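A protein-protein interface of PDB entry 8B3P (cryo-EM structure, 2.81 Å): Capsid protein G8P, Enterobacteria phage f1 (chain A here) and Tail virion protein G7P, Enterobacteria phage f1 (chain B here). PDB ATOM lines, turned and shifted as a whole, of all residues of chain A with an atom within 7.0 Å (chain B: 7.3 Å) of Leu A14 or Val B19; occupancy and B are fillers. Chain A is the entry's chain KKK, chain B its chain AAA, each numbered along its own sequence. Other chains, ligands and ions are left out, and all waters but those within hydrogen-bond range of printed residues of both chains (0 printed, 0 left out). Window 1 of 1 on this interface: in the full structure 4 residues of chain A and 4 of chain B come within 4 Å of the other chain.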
ATOM      1  N   ALA A   7     -11.072 -15.342  28.122  1.00  0.00           N
ATOM      2  CA  ALA A   7     -12.162 -16.302  28.013  1.00  0.00           C
ATOM      3  C   ALA A   7     -13.495 -15.666  28.409  1.00  0.00           C
ATOM      4  O   ALA A   7     -14.526 -15.976  27.809  1.00  0.00           O
ATOM      5  CB  ALA A   7     -11.863 -17.518  28.853  1.00  0.00           C
ATOM      6  N   ALA A   9     -14.089 -12.489  27.862  1.00  0.00           N
ATOM      7  CA  ALA A   9     -14.300 -11.691  26.661  1.00  0.00           C
ATOM      8  C   ALA A   9     -14.948 -12.525  25.553  1.00  0.00           C
ATOM      9  O   ALA A   9     -15.895 -12.066  24.910  1.00  0.00           O
ATOM     10  CB  ALA A   9     -12.995 -11.076  26.210  1.00  0.00           C
ATOM     11  N   ALA A  10     -14.439 -13.752  25.363  1.00  0.00           N
ATOM     12  CA  ALA A  10     -14.930 -14.691  24.364  1.00  0.00           C
ATOM     13  C   ALA A  10     -16.419 -14.971  24.569  1.00  0.00           C
ATOM     14  O   ALA A  10     -17.195 -14.848  23.626  1.00  0.00           O
ATOM     15  CB  ALA A  10     -14.116 -15.964  24.379  1.00  0.00           C
ATOM     16  N   PHE A  11     -16.803 -15.327  25.801  1.00  0.00           N
ATOM     17  CA  PHE A  11     -18.181 -15.664  26.120  1.00  0.00           C
ATOM     18  C   PHE A  11     -19.094 -14.458  25.893  1.00  0.00           C
ATOM     19  O   PHE A  11     -20.211 -14.623  25.417  1.00  0.00           O
ATOM     20  CB  PHE A  11     -18.286 -16.247  27.533  1.00  0.00           C
ATOM     21  CG  PHE A  11     -19.692 -16.497  28.021  1.00  0.00           C
ATOM     22  CD1 PHE A  11     -20.453 -17.548  27.520  1.00  0.00           C
ATOM     23  CD2 PHE A  11     -20.253 -15.686  28.998  1.00  0.00           C
ATOM     24  CE1 PHE A  11     -21.751 -17.763  27.965  1.00  0.00           C
ATOM     25  CE2 PHE A  11     -21.548 -15.904  29.446  1.00  0.00           C
ATOM     26  CZ  PHE A  11     -22.298 -16.939  28.928  1.00  0.00           C
ATOM     27  N   ASP A  12     -18.611 -13.253  26.222  1.00  0.00           N
ATOM     28  CA  ASP A  12     -19.404 -12.039  26.089  1.00  0.00           C
ATOM     29  C   ASP A  12     -19.745 -11.771  24.624  1.00  0.00           C
ATOM     30  O   ASP A  12     -20.866 -11.369  24.317  1.00  0.00           O
ATOM     31  CB  ASP A  12     -18.726 -10.833  26.742  1.00  0.00           C
ATOM     32  CG  ASP A  12     -18.641 -10.920  28.259  1.00  0.00           C
ATOM     33  OD1 ASP A  12     -19.374 -11.739  28.854  1.00  0.00           O
ATOM     34  OD2 ASP A  12     -17.837 -10.164  28.838  1.00  0.00           O
ATOM     35  N   SER A  13     -18.778 -12.013  23.730  1.00  0.00           N
ATOM     36  CA  SER A  13     -18.977 -11.782  22.307  1.00  0.00           C
ATOM     37  C   SER A  13     -19.967 -12.796  21.725  1.00  0.00           C
ATOM     38  O   SER A  13     -20.803 -12.434  20.889  1.00  0.00           O
ATOM     39  CB  SER A  13     -17.667 -11.783  21.566  1.00  0.00           C
ATOM     40  OG  SER A  13     -17.236 -13.110  21.307  1.00  0.00           O
ATOM     41  N   LEU A  14     -19.855 -14.053  22.190  1.00  0.00           N
ATOM     42  CA  LEU A  14     -20.714 -15.143  21.761  1.00  0.00           C
ATOM     43  C   LEU A  14     -22.162 -14.805  22.080  1.00  0.00           C
ATOM     44  O   LEU A  14     -22.997 -15.054  21.233  1.00  0.00           O
ATOM     45  CB  LEU A  14     -20.326 -16.481  22.406  1.00  0.00           C
ATOM     46  CG  LEU A  14     -21.292 -17.640  22.114  1.00  0.00           C
ATOM     47  CD1 LEU A  14     -21.088 -18.219  20.719  1.00  0.00           C
ATOM     48  CD2 LEU A  14     -21.251 -18.729  23.178  1.00  0.00           C
ATOM     49  N   GLN A  15     -22.433 -14.278  23.286  1.00  0.00           N
ATOM     50  CA  GLN A  15     -23.788 -14.000  23.736  1.00  0.00           C
ATOM     51  C   GLN A  15     -24.516 -13.103  22.739  1.00  0.00           C
ATOM     52  O   GLN A  15     -25.692 -13.345  22.473  1.00  0.00           O
ATOM     53  CB  GLN A  15     -23.819 -13.382  25.137  1.00  0.00           C
ATOM     54  CG  GLN A  15     -23.731 -14.393  26.274  1.00  0.00           C
ATOM     55  CD  GLN A  15     -24.567 -14.003  27.470  1.00  0.00           C
ATOM     56  OE1 GLN A  15     -24.052 -13.592  28.508  1.00  0.00           O
ATOM     57  NE2 GLN A  15     -25.880 -14.116  27.330  1.00  0.00           N
ATOM     58  N   ALA A  16     -23.816 -12.084  22.207  1.00  0.00           N
ATOM     59  CA  ALA A  16     -24.430 -11.120  21.298  1.00  0.00           C
ATOM     60  C   ALA A  16     -24.907 -11.787  20.001  1.00  0.00           C
ATOM     61  O   ALA A  16     -26.052 -11.596  19.563  1.00  0.00           O
ATOM     62  CB  ALA A  16     -23.482  -9.971  21.035  1.00  0.00           C
ATOM     63  N   SER A  17     -24.009 -12.584  19.405  1.00  0.00           N
ATOM     64  CA  SER A  17     -24.267 -13.292  18.161  1.00  0.00           C
ATOM     65  C   SER A  17     -25.424 -14.279  18.325  1.00  0.00           C
ATOM     66  O   SER A  17     -26.263 -14.385  17.436  1.00  0.00           O
ATOM     67  CB  SER A  17     -23.016 -13.970  17.655  1.00  0.00           C
ATOM     68  OG  SER A  17     -22.714 -15.130  18.419  1.00  0.00           O
ATOM     69  N   ALA A  18     -25.460 -14.972  19.474  1.00  0.00           N
ATOM     70  CA  ALA A  18     -26.464 -15.982  19.770  1.00  0.00           C
ATOM     71  C   ALA A  18     -27.841 -15.344  19.901  1.00  0.00           C
ATOM     72  O   ALA A  18     -28.815 -15.954  19.481  1.00  0.00           O
ATOM     73  CB  ALA A  18     -26.110 -16.756  21.015  1.00  0.00           C
ATOM     74  N   THR A  19     -27.903 -14.125  20.451  1.00  0.00           N
ATOM     75  CA  THR A  19     -29.167 -13.434  20.658  1.00  0.00           C
ATOM     76  C   THR A  19     -29.823 -13.113  19.318  1.00  0.00           C
ATOM     77  O   THR A  19     -31.042 -13.222  19.201  1.00  0.00           O
ATOM     78  CB  THR A  19     -28.977 -12.225  21.582  1.00  0.00           C
ATOM     79  OG1 THR A  19     -28.431 -12.769  22.784  1.00  0.00           O
ATOM     80  CG2 THR A  19     -30.262 -11.493  21.902  1.00  0.00           C
ATOM     81  N   ALA B  13      -6.911 -18.696  19.919  1.00  0.00           N
ATOM     82  CA  ALA B  13      -7.679 -19.450  18.938  1.00  0.00           C
ATOM     83  C   ALA B  13      -8.424 -20.591  19.622  1.00  0.00           C
ATOM     84  O   ALA B  13      -9.626 -20.738  19.419  1.00  0.00           O
ATOM     85  CB  ALA B  13      -6.799 -19.949  17.817  1.00  0.00           C
ATOM     86  N   MET B  14      -7.712 -21.358  20.459  1.00  0.00           N
ATOM     87  CA  MET B  14      -8.286 -22.509  21.141  1.00  0.00           C
ATOM     88  C   MET B  14      -9.545 -22.103  21.904  1.00  0.00           C
ATOM     89  O   MET B  14     -10.599 -22.696  21.691  1.00  0.00           O
ATOM     90  CB  MET B  14      -7.280 -23.167  22.088  1.00  0.00           C
ATOM     91  CG  MET B  14      -6.334 -24.114  21.375  1.00  0.00           C
ATOM     92  SD  MET B  14      -5.370 -25.123  22.527  1.00  0.00           S
ATOM     93  CE  MET B  14      -4.328 -23.853  23.239  1.00  0.00           C
ATOM     94  N   ILE B  15      -9.430 -21.062  22.739  1.00  0.00           N
ATOM     95  CA  ILE B  15     -10.532 -20.575  23.556  1.00  0.00           C
ATOM     96  C   ILE B  15     -11.734 -20.237  22.672  1.00  0.00           C
ATOM     97  O   ILE B  15     -12.851 -20.661  22.971  1.00  0.00           O
ATOM     98  CB  ILE B  15     -10.092 -19.391  24.444  1.00  0.00           C
ATOM     99  CG1 ILE B  15      -8.943 -19.794  25.375  1.00  0.00           C
ATOM    100  CG2 ILE B  15     -11.279 -18.821  25.214  1.00  0.00           C
ATOM    101  CD1 ILE B  15      -8.521 -18.720  26.354  1.00  0.00           C
ATOM    102  N   GLN B  16     -11.487 -19.508  21.573  1.00  0.00           N
ATOM    103  CA  GLN B  16     -12.545 -19.022  20.697  1.00  0.00           C
ATOM    104  C   GLN B  16     -13.314 -20.185  20.065  1.00  0.00           C
ATOM    105  O   GLN B  16     -14.543 -20.198  20.122  1.00  0.00           O
ATOM    106  CB  GLN B  16     -12.016 -18.003  19.686  1.00  0.00           C
ATOM    107  CG  GLN B  16     -12.079 -16.569  20.192  1.00  0.00           C
ATOM    108  CD  GLN B  16     -10.935 -15.715  19.699  1.00  0.00           C
ATOM    109  OE1 GLN B  16     -10.780 -15.477  18.503  1.00  0.00           O
ATOM    110  NE2 GLN B  16     -10.130 -15.229  20.630  1.00  0.00           N
ATOM    111  N   ILE B  17     -12.591 -21.174  19.519  1.00  0.00           N
ATOM    112  CA  ILE B  17     -13.200 -22.343  18.896  1.00  0.00           C
ATOM    113  C   ILE B  17     -14.007 -23.134  19.934  1.00  0.00           C
ATOM    114  O   ILE B  17     -15.132 -23.541  19.653  1.00  0.00           O
ATOM    115  CB  ILE B  17     -12.160 -23.200  18.136  1.00  0.00           C
ATOM    116  CG1 ILE B  17     -11.454 -22.389  17.042  1.00  0.00           C
ATOM    117  CG2 ILE B  17     -12.796 -24.467  17.576  1.00  0.00           C
ATOM    118  CD1 ILE B  17     -10.209 -23.044  16.456  1.00  0.00           C
ATOM    119  N   SER B  18     -13.448 -23.302  21.143  1.00  0.00           N
ATOM    120  CA  SER B  18     -14.061 -24.046  22.239  1.00  0.00           C
ATOM    121  C   SER B  18     -15.457 -23.527  22.577  1.00  0.00           C
ATOM    122  O   SER B  18     -16.396 -24.314  22.671  1.00  0.00           O
ATOM    123  CB  SER B  18     -13.177 -24.056  23.455  1.00  0.00           C
ATOM    124  OG  SER B  18     -12.137 -25.002  23.276  1.00  0.00           O
ATOM    125  N   VAL B  19     -15.574 -22.205  22.750  1.00  0.00           N
ATOM    126  CA  VAL B  19     -16.818 -21.552  23.132  1.00  0.00           C
ATOM    127  C   VAL B  19     -17.913 -21.874  22.109  1.00  0.00           C
ATOM    128  O   VAL B  19     -19.005 -22.281  22.501  1.00  0.00           O
ATOM    129  CB  VAL B  19     -16.602 -20.044  23.383  1.00  0.00           C
ATOM    130  CG1 VAL B  19     -17.895 -19.284  23.622  1.00  0.00           C
ATOM    131  CG2 VAL B  19     -15.651 -19.810  24.550  1.00  0.00           C
ATOM    132  N   VAL B  20     -17.591 -21.766  20.811  1.00  0.00           N
ATOM    133  CA  VAL B  20     -18.552 -21.998  19.737  1.00  0.00           C
ATOM    134  C   VAL B  20     -18.955 -23.474  19.681  1.00  0.00           C
ATOM    135  O   VAL B  20     -20.128 -23.766  19.452  1.00  0.00           O
ATOM    136  CB  VAL B  20     -18.057 -21.473  18.371  1.00  0.00           C
ATOM    137  CG1 VAL B  20     -19.074 -21.690  17.256  1.00  0.00           C
ATOM    138  CG2 VAL B  20     -17.665 -20.004  18.438  1.00  0.00           C
ATOM    139  N   LEU B  21     -18.000 -24.394  19.904  1.00  0.00           N
ATOM    140  CA  LEU B  21     -18.285 -25.819  19.772  1.00  0.00           C
ATOM    141  C   LEU B  21     -19.197 -26.311  20.898  1.00  0.00           C
ATOM    142  O   LEU B  21     -19.961 -27.253  20.691  1.00  0.00           O
ATOM    143  CB  LEU B  21     -16.997 -26.649  19.706  1.00  0.00           C
ATOM    144  CG  LEU B  21     -16.277 -26.733  18.356  1.00  0.00           C
ATOM    145  CD1 LEU B  21     -15.096 -27.688  18.445  1.00  0.00           C
ATOM    146  CD2 LEU B  21     -17.206 -27.159  17.229  1.00  0.00           C
ATOM    147  N   CYS B  22     -19.128 -25.667  22.072  1.00  0.00           N
ATOM    148  CA  CYS B  22     -19.947 -26.076  23.206  1.00  0.00           C
ATOM    149  C   CYS B  22     -21.349 -25.479  23.115  1.00  0.00           C
ATOM    150  O   CYS B  22     -22.274 -25.992  23.743  1.00  0.00           O
ATOM    151  CB  CYS B  22     -19.291 -25.715  24.531  1.00  0.00           C
ATOM    152  SG  CYS B  22     -17.665 -26.485  24.733  1.00  0.00           S
ATOM    153  N   PHE B  23     -21.488 -24.393  22.341  1.00  0.00           N
ATOM    154  CA  PHE B  23     -22.778 -23.787  22.049  1.00  0.00           C
ATOM    155  C   PHE B  23     -23.584 -24.704  21.128  1.00  0.00           C
ATOM    156  O   PHE B  23     -24.769 -24.933  21.370  1.00  0.00           O
ATOM    157  CB  PHE B  23     -22.605 -22.373  21.484  1.00  0.00           C
ATOM    158  CG  PHE B  23     -23.906 -21.664  21.202  1.00  0.00           C
ATOM    159  CD1 PHE B  23     -24.614 -21.038  22.222  1.00  0.00           C
ATOM    160  CD2 PHE B  23     -24.443 -21.648  19.918  1.00  0.00           C
ATOM    161  CE1 PHE B  23     -25.823 -20.405  21.963  1.00  0.00           C
ATOM    162  CE2 PHE B  23     -25.655 -21.019  19.660  1.00  0.00           C
ATOM    163  CZ  PHE B  23     -26.339 -20.394  20.683  1.00  0.00           C
ATOM    164  N   ALA B  24     -22.919 -25.229  20.086  1.00  0.00           N
ATOM    165  CA  ALA B  24     -23.539 -26.037  19.045  1.00  0.00           C
ATOM    166  C   ALA B  24     -24.044 -27.365  19.615  1.00  0.00           C
ATOM    167  O   ALA B  24     -25.134 -27.818  19.263  1.00  0.00           O
ATOM    168  CB  ALA B  24     -22.565 -26.243  17.911  1.00  0.00           C
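The backbone carbonyl oxygen of Leu A14 lies within hydrogen-bond range of the side-chain hydroxyl of Ser A17, 2.8 Å away.
Among the printed residues, pairs that only touch across the chains: Ala A7 with Ile B15 (3.9 Å), Leu A14 with Val B19 (3.4 Å) and Ala A18 with Phe B23 (3.7 Å).
Printed residues of chain B within 4 Å of Ala A7: Ile B15 (3.9 Å). No residue of chain B comes within 4 Å of Ser A13. Of the printed residues of chain B, Leu A14 touches Val B19. Of the printed residues of chain A, Ile B15 touches Ala A7 (3.9 Å). Val B19 touches just one residue of chain A: Leu A14. Of the printed residues of chain A, Phe B23 touches Ala A18 (3.7 Å). The nearest residue of chain B that does not touch Leu A14 is Phe B23 (4.2 Å).
Hydrophobic or aromatic side chains of chain A within 4 Å of the printed part of chain B: Ala A7, Leu A14 and Ala A18. Along chain A the printed residues that touch a printed residue of chain B span positions 7 to 18. Hydrophobic or aromatic side chains of chain B that line the printed part of chain A: Ile B15, Val B19 and Phe B23. Among the printed residues, 3 pairs touch across the chains. Among the printed residues, no Asp or Glu carboxylate lies within 4 Å of a Lys or Arg side-chain nitrogen of the other chain.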
